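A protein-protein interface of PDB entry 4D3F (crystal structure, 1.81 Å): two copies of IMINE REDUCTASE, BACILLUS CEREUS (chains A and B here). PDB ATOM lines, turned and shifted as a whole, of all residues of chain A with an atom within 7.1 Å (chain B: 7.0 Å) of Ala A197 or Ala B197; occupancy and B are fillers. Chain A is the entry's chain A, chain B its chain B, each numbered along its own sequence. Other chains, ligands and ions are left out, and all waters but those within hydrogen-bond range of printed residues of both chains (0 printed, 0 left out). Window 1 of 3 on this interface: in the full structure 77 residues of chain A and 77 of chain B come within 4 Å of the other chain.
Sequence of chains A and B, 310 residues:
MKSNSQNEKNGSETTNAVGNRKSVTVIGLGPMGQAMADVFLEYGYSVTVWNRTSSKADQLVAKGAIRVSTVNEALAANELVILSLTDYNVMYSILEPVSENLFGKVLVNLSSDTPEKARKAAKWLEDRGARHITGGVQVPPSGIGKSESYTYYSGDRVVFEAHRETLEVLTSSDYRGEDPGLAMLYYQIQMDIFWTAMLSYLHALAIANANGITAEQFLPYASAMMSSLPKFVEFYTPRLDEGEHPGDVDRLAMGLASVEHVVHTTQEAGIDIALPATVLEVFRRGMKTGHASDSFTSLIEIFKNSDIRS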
ATOM      1  N   MET A 191     -20.182  12.387   8.077  1.00  0.00           N
ATOM      2  CA  MET A 191     -19.172  13.411   8.124  1.00  0.00           C
ATOM      3  C   MET A 191     -19.732  14.807   7.854  1.00  0.00           C
ATOM      4  O   MET A 191     -19.205  15.812   8.385  1.00  0.00           O
ATOM      5  CB  MET A 191     -18.012  13.053   7.153  1.00  0.00           C
ATOM      6  CG  MET A 191     -17.293  11.774   7.563  1.00  0.00           C
ATOM      7  SD  MET A 191     -16.707  11.742   9.286  1.00  0.00           S
ATOM      8  CE  MET A 191     -15.635  13.104   9.222  1.00  0.00           C
ATOM      9  N   ASP A 192     -20.791  14.913   7.042  1.00  0.00           N
ATOM     10  CA  ASP A 192     -21.513  16.144   6.853  1.00  0.00           C
ATOM     11  C   ASP A 192     -21.958  16.720   8.239  1.00  0.00           C
ATOM     12  O   ASP A 192     -21.683  17.902   8.538  1.00  0.00           O
ATOM     13  CB  ASP A 192     -22.690  15.881   5.968  1.00  0.00           C
ATOM     14  CG  ASP A 192     -23.359  17.107   5.382  1.00  0.00           C
ATOM     15  OD1 ASP A 192     -22.854  18.251   5.447  1.00  0.00           O
ATOM     16  OD2 ASP A 192     -24.488  16.874   4.776  1.00  0.00           O
ATOM     17  N   ILE A 193     -22.510  15.883   9.048  1.00  0.00           N
ATOM     18  CA  ILE A 193     -22.937  16.314  10.417  1.00  0.00           C
ATOM     19  C   ILE A 193     -21.717  16.605  11.259  1.00  0.00           C
ATOM     20  O   ILE A 193     -21.647  17.637  11.947  1.00  0.00           O
ATOM     21  CB  ILE A 193     -23.815  15.242  11.076  1.00  0.00           C
ATOM     22  CG1 ILE A 193     -25.175  15.100  10.338  1.00  0.00           C
ATOM     23  CG2 ILE A 193     -24.047  15.599  12.574  1.00  0.00           C
ATOM     24  CD1 ILE A 193     -26.051  13.949  10.790  1.00  0.00           C
ATOM     25  N   PHE A 194     -20.726  15.682  11.260  1.00  0.00           N
ATOM     26  CA  PHE A 194     -19.566  15.900  12.136  1.00  0.00           C
ATOM     27  C   PHE A 194     -18.911  17.239  11.894  1.00  0.00           C
ATOM     28  O   PHE A 194     -18.673  18.021  12.812  1.00  0.00           O
ATOM     29  CB  PHE A 194     -18.522  14.766  11.988  1.00  0.00           C
ATOM     30  CG  PHE A 194     -17.290  14.976  12.847  1.00  0.00           C
ATOM     31  CD1 PHE A 194     -17.264  14.534  14.135  1.00  0.00           C
ATOM     32  CD2 PHE A 194     -16.202  15.655  12.340  1.00  0.00           C
ATOM     33  CE1 PHE A 194     -16.125  14.739  14.939  1.00  0.00           C
ATOM     34  CE2 PHE A 194     -15.112  15.913  13.141  1.00  0.00           C
ATOM     35  CZ  PHE A 194     -15.080  15.437  14.450  1.00  0.00           C
ATOM     36  N   TRP A 195     -18.574  17.556  10.629  1.00  0.00           N
ATOM     37  CA  TRP A 195     -17.799  18.737  10.404  1.00  0.00           C
ATOM     38  C   TRP A 195     -18.596  20.017  10.624  1.00  0.00           C
ATOM     39  O   TRP A 195     -18.058  21.043  11.108  1.00  0.00           O
ATOM     40  CB  TRP A 195     -17.211  18.749   8.972  1.00  0.00           C
ATOM     41  CG  TRP A 195     -16.152  17.720   8.752  1.00  0.00           C
ATOM     42  CD1 TRP A 195     -16.149  16.753   7.780  1.00  0.00           C
ATOM     43  CD2 TRP A 195     -14.910  17.605   9.455  1.00  0.00           C
ATOM     44  NE1 TRP A 195     -14.974  16.019   7.871  1.00  0.00           N
ATOM     45  CE2 TRP A 195     -14.228  16.483   8.917  1.00  0.00           C
ATOM     46  CE3 TRP A 195     -14.283  18.365  10.459  1.00  0.00           C
ATOM     47  CZ2 TRP A 195     -12.941  16.131   9.348  1.00  0.00           C
ATOM     48  CZ3 TRP A 195     -12.999  17.956  10.945  1.00  0.00           C
ATOM     49  CH2 TRP A 195     -12.366  16.874  10.373  1.00  0.00           C
ATOM     50  N   THR A 196     -19.865  19.982  10.234  1.00  0.00           N
ATOM     51  CA  THR A 196     -20.656  21.192  10.305  1.00  0.00           C
ATOM     52  C   THR A 196     -20.942  21.458  11.806  1.00  0.00           C
ATOM     53  O   THR A 196     -20.891  22.572  12.263  1.00  0.00           O
ATOM     54  CB  THR A 196     -21.972  21.054   9.522  1.00  0.00           C
ATOM     55  OG1 THR A 196     -21.682  20.643   8.166  1.00  0.00           O
ATOM     56  CG2 THR A 196     -22.660  22.374   9.497  1.00  0.00           C
ATOM     57  N   ALA A 197     -21.304  20.443  12.540  1.00  0.00           N
ATOM     58  CA  ALA A 197     -21.650  20.593  13.972  1.00  0.00           C
ATOM     59  C   ALA A 197     -20.408  20.943  14.785  1.00  0.00           C
ATOM     60  O   ALA A 197     -20.460  21.840  15.650  1.00  0.00           O
ATOM     61  CB  ALA A 197     -22.287  19.356  14.491  1.00  0.00           C
ATOM     62  N   MET A 198     -19.238  20.322  14.491  1.00  0.00           N
ATOM     63  CA  MET A 198     -18.011  20.732  15.194  1.00  0.00           C
ATOM     64  C   MET A 198     -17.553  22.097  14.908  1.00  0.00           C
ATOM     65  O   MET A 198     -17.111  22.836  15.773  1.00  0.00           O
ATOM     66  CB  MET A 198     -16.867  19.722  14.955  1.00  0.00           C
ATOM     67  CG  MET A 198     -17.170  18.414  15.577  1.00  0.00           C
ATOM     68  SD  MET A 198     -17.380  18.441  17.440  1.00  0.00           S
ATOM     69  CE  MET A 198     -15.823  19.062  17.996  1.00  0.00           C
ATOM     70  N   LEU A 199     -17.688  22.573  13.675  1.00  0.00           N
ATOM     71  CA  LEU A 199     -17.437  23.951  13.406  1.00  0.00           C
ATOM     72  C   LEU A 199     -18.380  24.886  14.135  1.00  0.00           C
ATOM     73  O   LEU A 199     -17.976  26.003  14.500  1.00  0.00           O
ATOM     74  CB  LEU A 199     -17.476  24.311  11.898  1.00  0.00           C
ATOM     75  CG  LEU A 199     -16.107  24.396  11.197  1.00  0.00           C
ATOM     76  CD1 LEU A 199     -15.278  23.182  11.409  1.00  0.00           C
ATOM     77  CD2 LEU A 199     -16.291  24.726   9.705  1.00  0.00           C
ATOM     78  N   SER A 200     -19.659  24.511  14.223  1.00  0.00           N
ATOM     79  CA  SER A 200     -20.606  25.338  15.024  1.00  0.00           C
ATOM     80  C   SER A 200     -20.167  25.468  16.468  1.00  0.00           C
ATOM     81  O   SER A 200     -20.320  26.573  17.049  1.00  0.00           O
ATOM     82  CB  SER A 200     -22.012  24.850  14.937  1.00  0.00           C
ATOM     83  OG  SER A 200     -22.379  23.751  15.756  1.00  0.00           O
ATOM     84  N   TYR A 201     -19.626  24.388  16.996  1.00  0.00           N
ATOM     85  CA  TYR A 201     -19.047  24.389  18.353  1.00  0.00           C
ATOM     86  C   TYR A 201     -17.878  25.368  18.442  1.00  0.00           C
ATOM     87  O   TYR A 201     -17.803  26.225  19.332  1.00  0.00           O
ATOM     88  CB  TYR A 201     -18.664  22.991  18.817  1.00  0.00           C
ATOM     89  CG  TYR A 201     -17.713  23.056  19.993  1.00  0.00           C
ATOM     90  CD1 TYR A 201     -18.182  23.359  21.298  1.00  0.00           C
ATOM     91  CD2 TYR A 201     -16.351  22.872  19.821  1.00  0.00           C
ATOM     92  CE1 TYR A 201     -17.303  23.448  22.363  1.00  0.00           C
ATOM     93  CE2 TYR A 201     -15.456  23.004  20.856  1.00  0.00           C
ATOM     94  CZ  TYR A 201     -15.917  23.300  22.135  1.00  0.00           C
ATOM     95  OH  TYR A 201     -15.005  23.390  23.199  1.00  0.00           O
ATOM     96  N   LEU A 202     -16.975  25.332  17.474  1.00  0.00           N
ATOM     97  CA  LEU A 202     -15.847  26.288  17.497  1.00  0.00           C
ATOM     98  C   LEU A 202     -16.340  27.731  17.340  1.00  0.00           C
ATOM     99  O   LEU A 202     -15.785  28.643  17.976  1.00  0.00           O
ATOM    100  CB  LEU A 202     -14.820  25.959  16.429  1.00  0.00           C
ATOM    101  CG  LEU A 202     -14.123  24.620  16.591  1.00  0.00           C
ATOM    102  CD1 LEU A 202     -13.277  24.351  15.334  1.00  0.00           C
ATOM    103  CD2 LEU A 202     -13.281  24.592  17.851  1.00  0.00           C
ATOM    104  N   HIS A 203     -17.306  27.954  16.438  1.00  0.00           N
ATOM    105  CA  HIS A 203     -17.902  29.248  16.251  1.00  0.00           C
ATOM    106  C   HIS A 203     -18.534  29.797  17.583  1.00  0.00           C
ATOM    107  O   HIS A 203     -18.285  30.947  17.963  1.00  0.00           O
ATOM    108  CB  HIS A 203     -18.927  29.201  15.159  1.00  0.00           C
ATOM    109  CG  HIS A 203     -19.441  30.513  14.799  1.00  0.00           C
ATOM    110  ND1 HIS A 203     -20.587  31.018  15.381  1.00  0.00           N
ATOM    111  CD2 HIS A 203     -19.023  31.432  13.901  1.00  0.00           C
ATOM    112  CE1 HIS A 203     -20.800  32.226  14.884  1.00  0.00           C
ATOM    113  NE2 HIS A 203     -19.857  32.489  13.991  1.00  0.00           N
ATOM    114  N   MET A 225     -26.029  20.209  24.927  1.00  0.00           N
ATOM    115  CA  MET A 225     -26.778  20.520  23.671  1.00  0.00           C
ATOM    116  C   MET A 225     -26.597  19.417  22.653  1.00  0.00           C
ATOM    117  O   MET A 225     -27.579  18.978  22.035  1.00  0.00           O
ATOM    118  CB  MET A 225     -26.362  21.851  23.136  1.00  0.00           C
ATOM    119  CG  MET A 225     -27.033  22.205  21.817  1.00  0.00           C
ATOM    120  SD  MET A 225     -28.831  22.182  21.876  1.00  0.00           S
ATOM    121  CE  MET A 225     -29.229  23.723  22.714  1.00  0.00           C
ATOM    122  N   MET A 226     -25.341  19.016  22.421  1.00  0.00           N
ATOM    123  CA  MET A 226     -25.068  17.932  21.474  1.00  0.00           C
ATOM    124  C   MET A 226     -25.781  16.696  21.828  1.00  0.00           C
ATOM    125  O   MET A 226     -26.367  16.033  20.989  1.00  0.00           O
ATOM    126  CB  MET A 226     -23.579  17.679  21.364  1.00  0.00           C
ATOM    127  CG  MET A 226     -22.918  18.833  20.672  1.00  0.00           C
ATOM    128  SD  MET A 226     -21.161  18.908  20.987  1.00  0.00           S
ATOM    129  CE  MET A 226     -20.778  20.085  19.677  1.00  0.00           C
ATOM    130  N   LEU A 229     -29.512  16.478  20.856  1.00  0.00           N
ATOM    131  CA  LEU A 229     -29.967  16.460  19.466  1.00  0.00           C
ATOM    132  C   LEU A 229     -30.609  15.137  18.997  1.00  0.00           C
ATOM    133  O   LEU A 229     -31.573  15.198  18.228  1.00  0.00           O
ATOM    134  CB  LEU A 229     -28.836  16.881  18.513  1.00  0.00           C
ATOM    135  CG  LEU A 229     -28.199  18.232  18.735  1.00  0.00           C
ATOM    136  CD1 LEU A 229     -27.090  18.509  17.776  1.00  0.00           C
ATOM    137  CD2 LEU A 229     -29.214  19.363  18.748  1.00  0.00           C
ATOM    138  N   LEU A 275     -20.645  31.343   8.841  1.00  0.00           N
ATOM    139  CA  LEU A 275     -21.369  30.142   9.147  1.00  0.00           C
ATOM    140  C   LEU A 275     -22.857  30.450   9.578  1.00  0.00           C
ATOM    141  O   LEU A 275     -23.804  29.934   8.982  1.00  0.00           O
ATOM    142  CB  LEU A 275     -20.594  29.359  10.157  1.00  0.00           C
ATOM    143  CG  LEU A 275     -21.198  27.985  10.501  1.00  0.00           C
ATOM    144  CD1 LEU A 275     -21.236  27.086   9.302  1.00  0.00           C
ATOM    145  CD2 LEU A 275     -20.402  27.350  11.607  1.00  0.00           C
ATOM    146  N   VAL A 279     -26.687  29.752   7.598  1.00  0.00           N
ATOM    147  CA  VAL A 279     -27.858  29.195   8.268  1.00  0.00           C
ATOM    148  C   VAL A 279     -29.056  30.137   8.096  1.00  0.00           C
ATOM    149  O   VAL A 279     -30.155  29.686   7.689  1.00  0.00           O
ATOM    150  CB  VAL A 279     -27.530  28.974   9.778  1.00  0.00           C
ATOM    151  CG1 VAL A 279     -28.728  28.519  10.573  1.00  0.00           C
ATOM    152  CG2 VAL A 279     -26.444  27.895   9.900  1.00  0.00           C
ATOM    153  N   MET B 191     -27.790  28.005  21.049  1.00  0.00           N
ATOM    154  CA  MET B 191     -28.686  28.007  19.860  1.00  0.00           C
ATOM    155  C   MET B 191     -27.856  28.052  18.562  1.00  0.00           C
ATOM    156  O   MET B 191     -28.365  27.518  17.516  1.00  0.00           O
ATOM    157  CB  MET B 191     -29.694  29.174  19.923  1.00  0.00           C
ATOM    158  CG  MET B 191     -30.678  29.046  21.110  1.00  0.00           C
ATOM    159  SD  MET B 191     -31.478  27.434  21.164  1.00  0.00           S
ATOM    160  CE  MET B 191     -32.381  27.602  19.662  1.00  0.00           C
ATOM    161  N   ASP B 192     -26.681  28.636  18.587  1.00  0.00           N
ATOM    162  CA  ASP B 192     -25.702  28.583  17.433  1.00  0.00           C
ATOM    163  C   ASP B 192     -25.438  27.135  17.101  1.00  0.00           C
ATOM    164  O   ASP B 192     -25.629  26.711  15.941  1.00  0.00           O
ATOM    165  CB  ASP B 192     -24.453  29.324  17.857  1.00  0.00           C
ATOM    166  CG  ASP B 192     -23.495  29.648  16.735  1.00  0.00           C
ATOM    167  OD1 ASP B 192     -23.856  29.517  15.527  1.00  0.00           O
ATOM    168  OD2 ASP B 192     -22.361  30.052  17.149  1.00  0.00           O
ATOM    169  N   ILE B 193     -25.149  26.325  18.098  1.00  0.00           N
ATOM    170  CA  ILE B 193     -24.936  24.908  17.868  1.00  0.00           C
ATOM    171  C   ILE B 193     -26.225  24.213  17.417  1.00  0.00           C
ATOM    172  O   ILE B 193     -26.267  23.426  16.440  1.00  0.00           O
ATOM    173  CB  ILE B 193     -24.365  24.179  19.121  1.00  0.00           C
ATOM    174  CG1 ILE B 193     -22.974  24.724  19.433  1.00  0.00           C
ATOM    175  CG2 ILE B 193     -24.339  22.689  18.918  1.00  0.00           C
ATOM    176  CD1 ILE B 193     -22.366  24.280  20.746  1.00  0.00           C
ATOM    177  N   PHE B 194     -27.329  24.427  18.178  1.00  0.00           N
ATOM    178  CA  PHE B 194     -28.601  23.759  17.807  1.00  0.00           C
ATOM    179  C   PHE B 194     -29.015  23.938  16.357  1.00  0.00           C
ATOM    180  O   PHE B 194     -29.274  22.935  15.656  1.00  0.00           O
ATOM    181  CB  PHE B 194     -29.768  24.222  18.704  1.00  0.00           C
ATOM    182  CG  PHE B 194     -31.071  23.527  18.373  1.00  0.00           C
ATOM    183  CD1 PHE B 194     -31.395  22.315  18.910  1.00  0.00           C
ATOM    184  CD2 PHE B 194     -31.971  24.094  17.484  1.00  0.00           C
ATOM    185  CE1 PHE B 194     -32.561  21.641  18.549  1.00  0.00           C
ATOM    186  CE2 PHE B 194     -33.136  23.443  17.136  1.00  0.00           C
ATOM    187  CZ  PHE B 194     -33.456  22.192  17.684  1.00  0.00           C
ATOM    188  N   TRP B 195     -29.089  25.167  15.925  1.00  0.00           N
ATOM    189  CA  TRP B 195     -29.631  25.406  14.575  1.00  0.00           C
ATOM    190  C   TRP B 195     -28.641  24.916  13.513  1.00  0.00           C
ATOM    191  O   TRP B 195     -29.052  24.354  12.457  1.00  0.00           O
ATOM    192  CB  TRP B 195     -29.934  26.829  14.355  1.00  0.00           C
ATOM    193  CG  TRP B 195     -31.125  27.309  15.104  1.00  0.00           C
ATOM    194  CD1 TRP B 195     -31.131  28.324  16.023  1.00  0.00           C
ATOM    195  CD2 TRP B 195     -32.442  26.820  15.031  1.00  0.00           C
ATOM    196  NE1 TRP B 195     -32.394  28.522  16.501  1.00  0.00           N
ATOM    197  CE2 TRP B 195     -33.230  27.626  15.922  1.00  0.00           C
ATOM    198  CE3 TRP B 195     -33.071  25.819  14.288  1.00  0.00           C
ATOM    199  CZ2 TRP B 195     -34.564  27.429  16.097  1.00  0.00           C
ATOM    200  CZ3 TRP B 195     -34.438  25.648  14.436  1.00  0.00           C
ATOM    201  CH2 TRP B 195     -35.175  26.463  15.340  1.00  0.00           C
ATOM    202  N   THR B 196     -27.371  25.130  13.763  1.00  0.00           N
ATOM    203  CA  THR B 196     -26.369  24.770  12.734  1.00  0.00           C
ATOM    204  C   THR B 196     -26.322  23.259  12.618  1.00  0.00           C
ATOM    205  O   THR B 196     -26.313  22.687  11.552  1.00  0.00           O
ATOM    206  CB  THR B 196     -25.002  25.409  13.028  1.00  0.00           C
ATOM    207  OG1 THR B 196     -25.139  26.818  13.186  1.00  0.00           O
ATOM    208  CG2 THR B 196     -24.046  25.181  11.837  1.00  0.00           C
ATOM    209  N   ALA B 197     -26.228  22.559  13.734  1.00  0.00           N
ATOM    210  CA  ALA B 197     -26.195  21.104  13.729  1.00  0.00           C
ATOM    211  C   ALA B 197     -27.472  20.484  13.235  1.00  0.00           C
ATOM    212  O   ALA B 197     -27.413  19.474  12.459  1.00  0.00           O
ATOM    213  CB  ALA B 197     -25.825  20.587  15.115  1.00  0.00           C
ATOM    214  N   MET B 198     -28.670  21.051  13.575  1.00  0.00           N
ATOM    215  CA  MET B 198     -29.886  20.485  13.054  1.00  0.00           C
ATOM    216  C   MET B 198     -30.035  20.720  11.551  1.00  0.00           C
ATOM    217  O   MET B 198     -30.560  19.836  10.845  1.00  0.00           O
ATOM    218  CB  MET B 198     -31.133  20.966  13.821  1.00  0.00           C
ATOM    219  CG  MET B 198     -31.142  20.394  15.283  1.00  0.00           C
ATOM    220  SD  MET B 198     -31.247  18.599  15.431  1.00  0.00           S
ATOM    221  CE  MET B 198     -32.704  18.188  14.540  1.00  0.00           C
ATOM    222  N   LEU B 199     -29.575  21.855  11.064  1.00  0.00           N
ATOM    223  CA  LEU B 199     -29.639  22.022   9.624  1.00  0.00           C
ATOM    224  C   LEU B 199     -28.660  21.018   8.918  1.00  0.00           C
ATOM    225  O   LEU B 199     -28.947  20.564   7.789  1.00  0.00           O
ATOM    226  CB  LEU B 199     -29.292  23.432   9.181  1.00  0.00           C
ATOM    227  CG  LEU B 199     -30.432  24.316   8.721  1.00  0.00           C
ATOM    228  CD1 LEU B 199     -31.490  24.330   9.793  1.00  0.00           C
ATOM    229  CD2 LEU B 199     -29.899  25.693   8.363  1.00  0.00           C
ATOM    230  N   SER B 200     -27.523  20.736   9.520  1.00  0.00           N
ATOM    231  CA  SER B 200     -26.602  19.704   8.977  1.00  0.00           C
ATOM    232  C   SER B 200     -27.226  18.361   8.892  1.00  0.00           C
ATOM    233  O   SER B 200     -27.038  17.618   7.903  1.00  0.00           O
ATOM    234  CB  SER B 200     -25.245  19.670   9.730  1.00  0.00           C
ATOM    235  OG  SER B 200     -25.267  18.898  10.930  1.00  0.00           O
ATOM    236  N   TYR B 201     -28.079  18.017   9.875  1.00  0.00           N
ATOM    237  CA  TYR B 201     -28.841  16.828   9.854  1.00  0.00           C
ATOM    238  C   TYR B 201     -29.801  16.845   8.698  1.00  0.00           C
ATOM    239  O   TYR B 201     -29.870  15.877   7.970  1.00  0.00           O
ATOM    240  CB  TYR B 201     -29.596  16.546  11.232  1.00  0.00           C
ATOM    241  CG  TYR B 201     -30.664  15.581  11.101  1.00  0.00           C
ATOM    242  CD1 TYR B 201     -30.387  14.214  11.007  1.00  0.00           C
ATOM    243  CD2 TYR B 201     -31.989  15.980  10.980  1.00  0.00           C
ATOM    244  CE1 TYR B 201     -31.388  13.306  10.758  1.00  0.00           C
ATOM    245  CE2 TYR B 201     -32.996  15.074  10.800  1.00  0.00           C
ATOM    246  CZ  TYR B 201     -32.718  13.756  10.692  1.00  0.00           C
ATOM    247  OH  TYR B 201     -33.686  12.862  10.473  1.00  0.00           O
ATOM    248  N   LEU B 202     -30.537  17.929   8.515  1.00  0.00           N
ATOM    249  CA  LEU B 202     -31.516  17.986   7.379  1.00  0.00           C
ATOM    250  C   LEU B 202     -30.767  17.884   6.029  1.00  0.00           C
ATOM    251  O   LEU B 202     -31.277  17.242   5.110  1.00  0.00           O
ATOM    252  CB  LEU B 202     -32.352  19.238   7.433  1.00  0.00           C
ATOM    253  CG  LEU B 202     -33.350  19.329   8.604  1.00  0.00           C
ATOM    254  CD1 LEU B 202     -33.993  20.703   8.544  1.00  0.00           C
ATOM    255  CD2 LEU B 202     -34.384  18.210   8.542  1.00  0.00           C
ATOM    256  N   HIS B 203     -29.632  18.558   5.934  1.00  0.00           N
ATOM    257  CA  HIS B 203     -28.792  18.531   4.693  1.00  0.00           C
ATOM    258  C   HIS B 203     -28.323  17.102   4.386  1.00  0.00           C
ATOM    259  O   HIS B 203     -28.501  16.595   3.269  1.00  0.00           O
ATOM    260  CB  HIS B 203     -27.618  19.470   4.884  1.00  0.00           C
ATOM    261  CG  HIS B 203     -26.805  19.605   3.641  1.00  0.00           C
ATOM    262  ND1 HIS B 203     -25.755  18.781   3.387  1.00  0.00           N
ATOM    263  CD2 HIS B 203     -26.955  20.397   2.553  1.00  0.00           C
ATOM    264  CE1 HIS B 203     -25.262  19.070   2.188  1.00  0.00           C
ATOM    265  NE2 HIS B 203     -25.982  20.050   1.665  1.00  0.00           N
ATOM    266  N   MET B 226     -24.166  12.263  16.531  1.00  0.00           N
ATOM    267  CA  MET B 226     -24.443  13.410  17.401  1.00  0.00           C
ATOM    268  C   MET B 226     -24.007  13.076  18.823  1.00  0.00           C
ATOM    269  O   MET B 226     -23.389  13.919  19.465  1.00  0.00           O
ATOM    270  CB  MET B 226     -25.896  13.782  17.390  1.00  0.00           C
ATOM    271  CG  MET B 226     -26.288  14.460  16.070  1.00  0.00           C
ATOM    272  SD  MET B 226     -28.052  14.402  15.800  1.00  0.00           S
ATOM    273  CE  MET B 226     -28.078  15.680  14.559  1.00  0.00           C
ATOM    274  N   LEU B 229     -20.278  13.526  19.651  1.00  0.00           N
ATOM    275  CA  LEU B 229     -19.633  14.783  19.627  1.00  0.00           C
ATOM    276  C   LEU B 229     -19.117  15.299  20.986  1.00  0.00           C
ATOM    277  O   LEU B 229     -18.081  15.932  21.021  1.00  0.00           O
ATOM    278  CB  LEU B 229     -20.464  15.836  18.946  1.00  0.00           C
ATOM    279  CG  LEU B 229     -20.895  15.538  17.506  1.00  0.00           C
ATOM    280  CD1 LEU B 229     -21.752  16.664  16.943  1.00  0.00           C
ATOM    281  CD2 LEU B 229     -19.714  15.233  16.611  1.00  0.00           C
ATOM    282  N   LEU B 275     -24.490  25.098   2.492  1.00  0.00           N
ATOM    283  CA  LEU B 275     -24.003  24.800   3.834  1.00  0.00           C
ATOM    284  C   LEU B 275     -22.581  24.097   3.847  1.00  0.00           C
ATOM    285  O   LEU B 275     -21.650  24.602   4.460  1.00  0.00           O
ATOM    286  CB  LEU B 275     -25.038  23.992   4.590  1.00  0.00           C
ATOM    287  CG  LEU B 275     -24.768  23.708   6.089  1.00  0.00           C
ATOM    288  CD1 LEU B 275     -24.638  25.004   6.892  1.00  0.00           C
ATOM    289  CD2 LEU B 275     -25.874  22.848   6.682  1.00  0.00           C
ATOM    290  N   VAL B 279     -18.661  25.521   5.052  1.00  0.00           N
ATOM    291  CA  VAL B 279     -17.749  24.730   5.832  1.00  0.00           C
ATOM    292  C   VAL B 279     -16.394  24.621   5.092  1.00  0.00           C
ATOM    293  O   VAL B 279     -15.299  24.864   5.685  1.00  0.00           O
ATOM    294  CB  VAL B 279     -18.334  23.357   6.132  1.00  0.00           C
ATOM    295  CG1 VAL B 279     -17.373  22.417   6.828  1.00  0.00           C
ATOM    296  CG2 VAL B 279     -19.589  23.497   7.048  1.00  0.00           C
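The side-chain carboxylate (OD2) of Asp A192 is in hydrogen-bond range of a ring nitrogen (ND1) of His B203 (2.7 Å). OD2 of Asp B192 lies within hydrogen-bond range of ND1 of His A203.
The backbone carbonyl oxygen of Asp A192 is in hydrogen-bond range of the side-chain hydroxyl of Thr A196, 2.8 Å away. The backbone carbonyl oxygen (O) of Ala A197 sits at hydrogen-bond distance from the side-chain hydroxyl (OG) of Ser A200 (2.7 Å). O of Ala B197 is in hydrogen-bond range of OG of Ser B200 (2.7 Å). O of Asp B192 sits at hydrogen-bond distance from OG1 of Thr B196, at 2.8 Å.
Ile A193 touches Ser B200 (CA to OG, 3.5 Å). Leu B229 touches Phe A194 (CD2 to CD1, 3.6 Å). CB of Thr A196 touches CB of Ser B200, 3.6 Å away. Thr A196 touches Val B279. Met A226 touches Met B226. SD of Met A226 touches CB of Leu B229, 3.8 Å away. CD2 of Leu A229 touches SD of Met B198, 3.96 Å away. Met B226 touches Leu A229 (SD to CB, 3.8 Å). Val A279 touches Thr B196. CG1 of Val A279 touches CD2 of Leu B199, at 3.8 Å.
Ala A197 touches just these residues of chain B: Ala B197 (3.8 Å) and Leu B229 (3.7 Å). Ala B197 touches two residues of chain A. Of the printed residues of chain B, Ile A193 touches Ser B200. Of the printed residues of chain B, Phe A194 touches Leu B229. Of the printed residues of chain B, Thr A196 touches Thr B196 (3.9 Å), Ser B200 (3.6 Å) and Val B279 (3.7 Å). Met A191 touches none of the printed residues of chain B. The nearest residue of chain B that does not touch Ala A197 is Ser B200 (4.5 Å). The nearest residue of chain A that does not touch Ala B197 is Ser A200 (4.5 Å).
Of the 18 printed residues of chain A, 12 touch a printed residue of chain B. Printed residues of chain A that touch a printed residue of chain B: Asp A192, Ile A193, Phe A194, Thr A196, Ala A197, Leu A199, Ser A200, His A203, Met A225, Met A226, Leu A229 and Val A279. Among the printed residues, 22 pairs touch across the chains. Among the printed residues, no Asp or Glu carboxylate lies within 4 Å of a Lys or Arg side-chain nitrogen of the other chain.
Thr A196 touches Val B279, and with the chains exchanged Val A279 touches Thr B196. Leu A199 touches Val B279, and with the chains exchanged Val A279 touches Leu B199. Met A226 touches Leu B229, and with the chains exchanged Leu A229 touches Met B226. Leu A229 touches Met B198, but with the chains exchanged Met A198 does not touch Leu B229 (4.1 Å). Of the 22 pairs that touch across the chains among the printed residues, 19 have their exchanged pair printed and touching as well.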
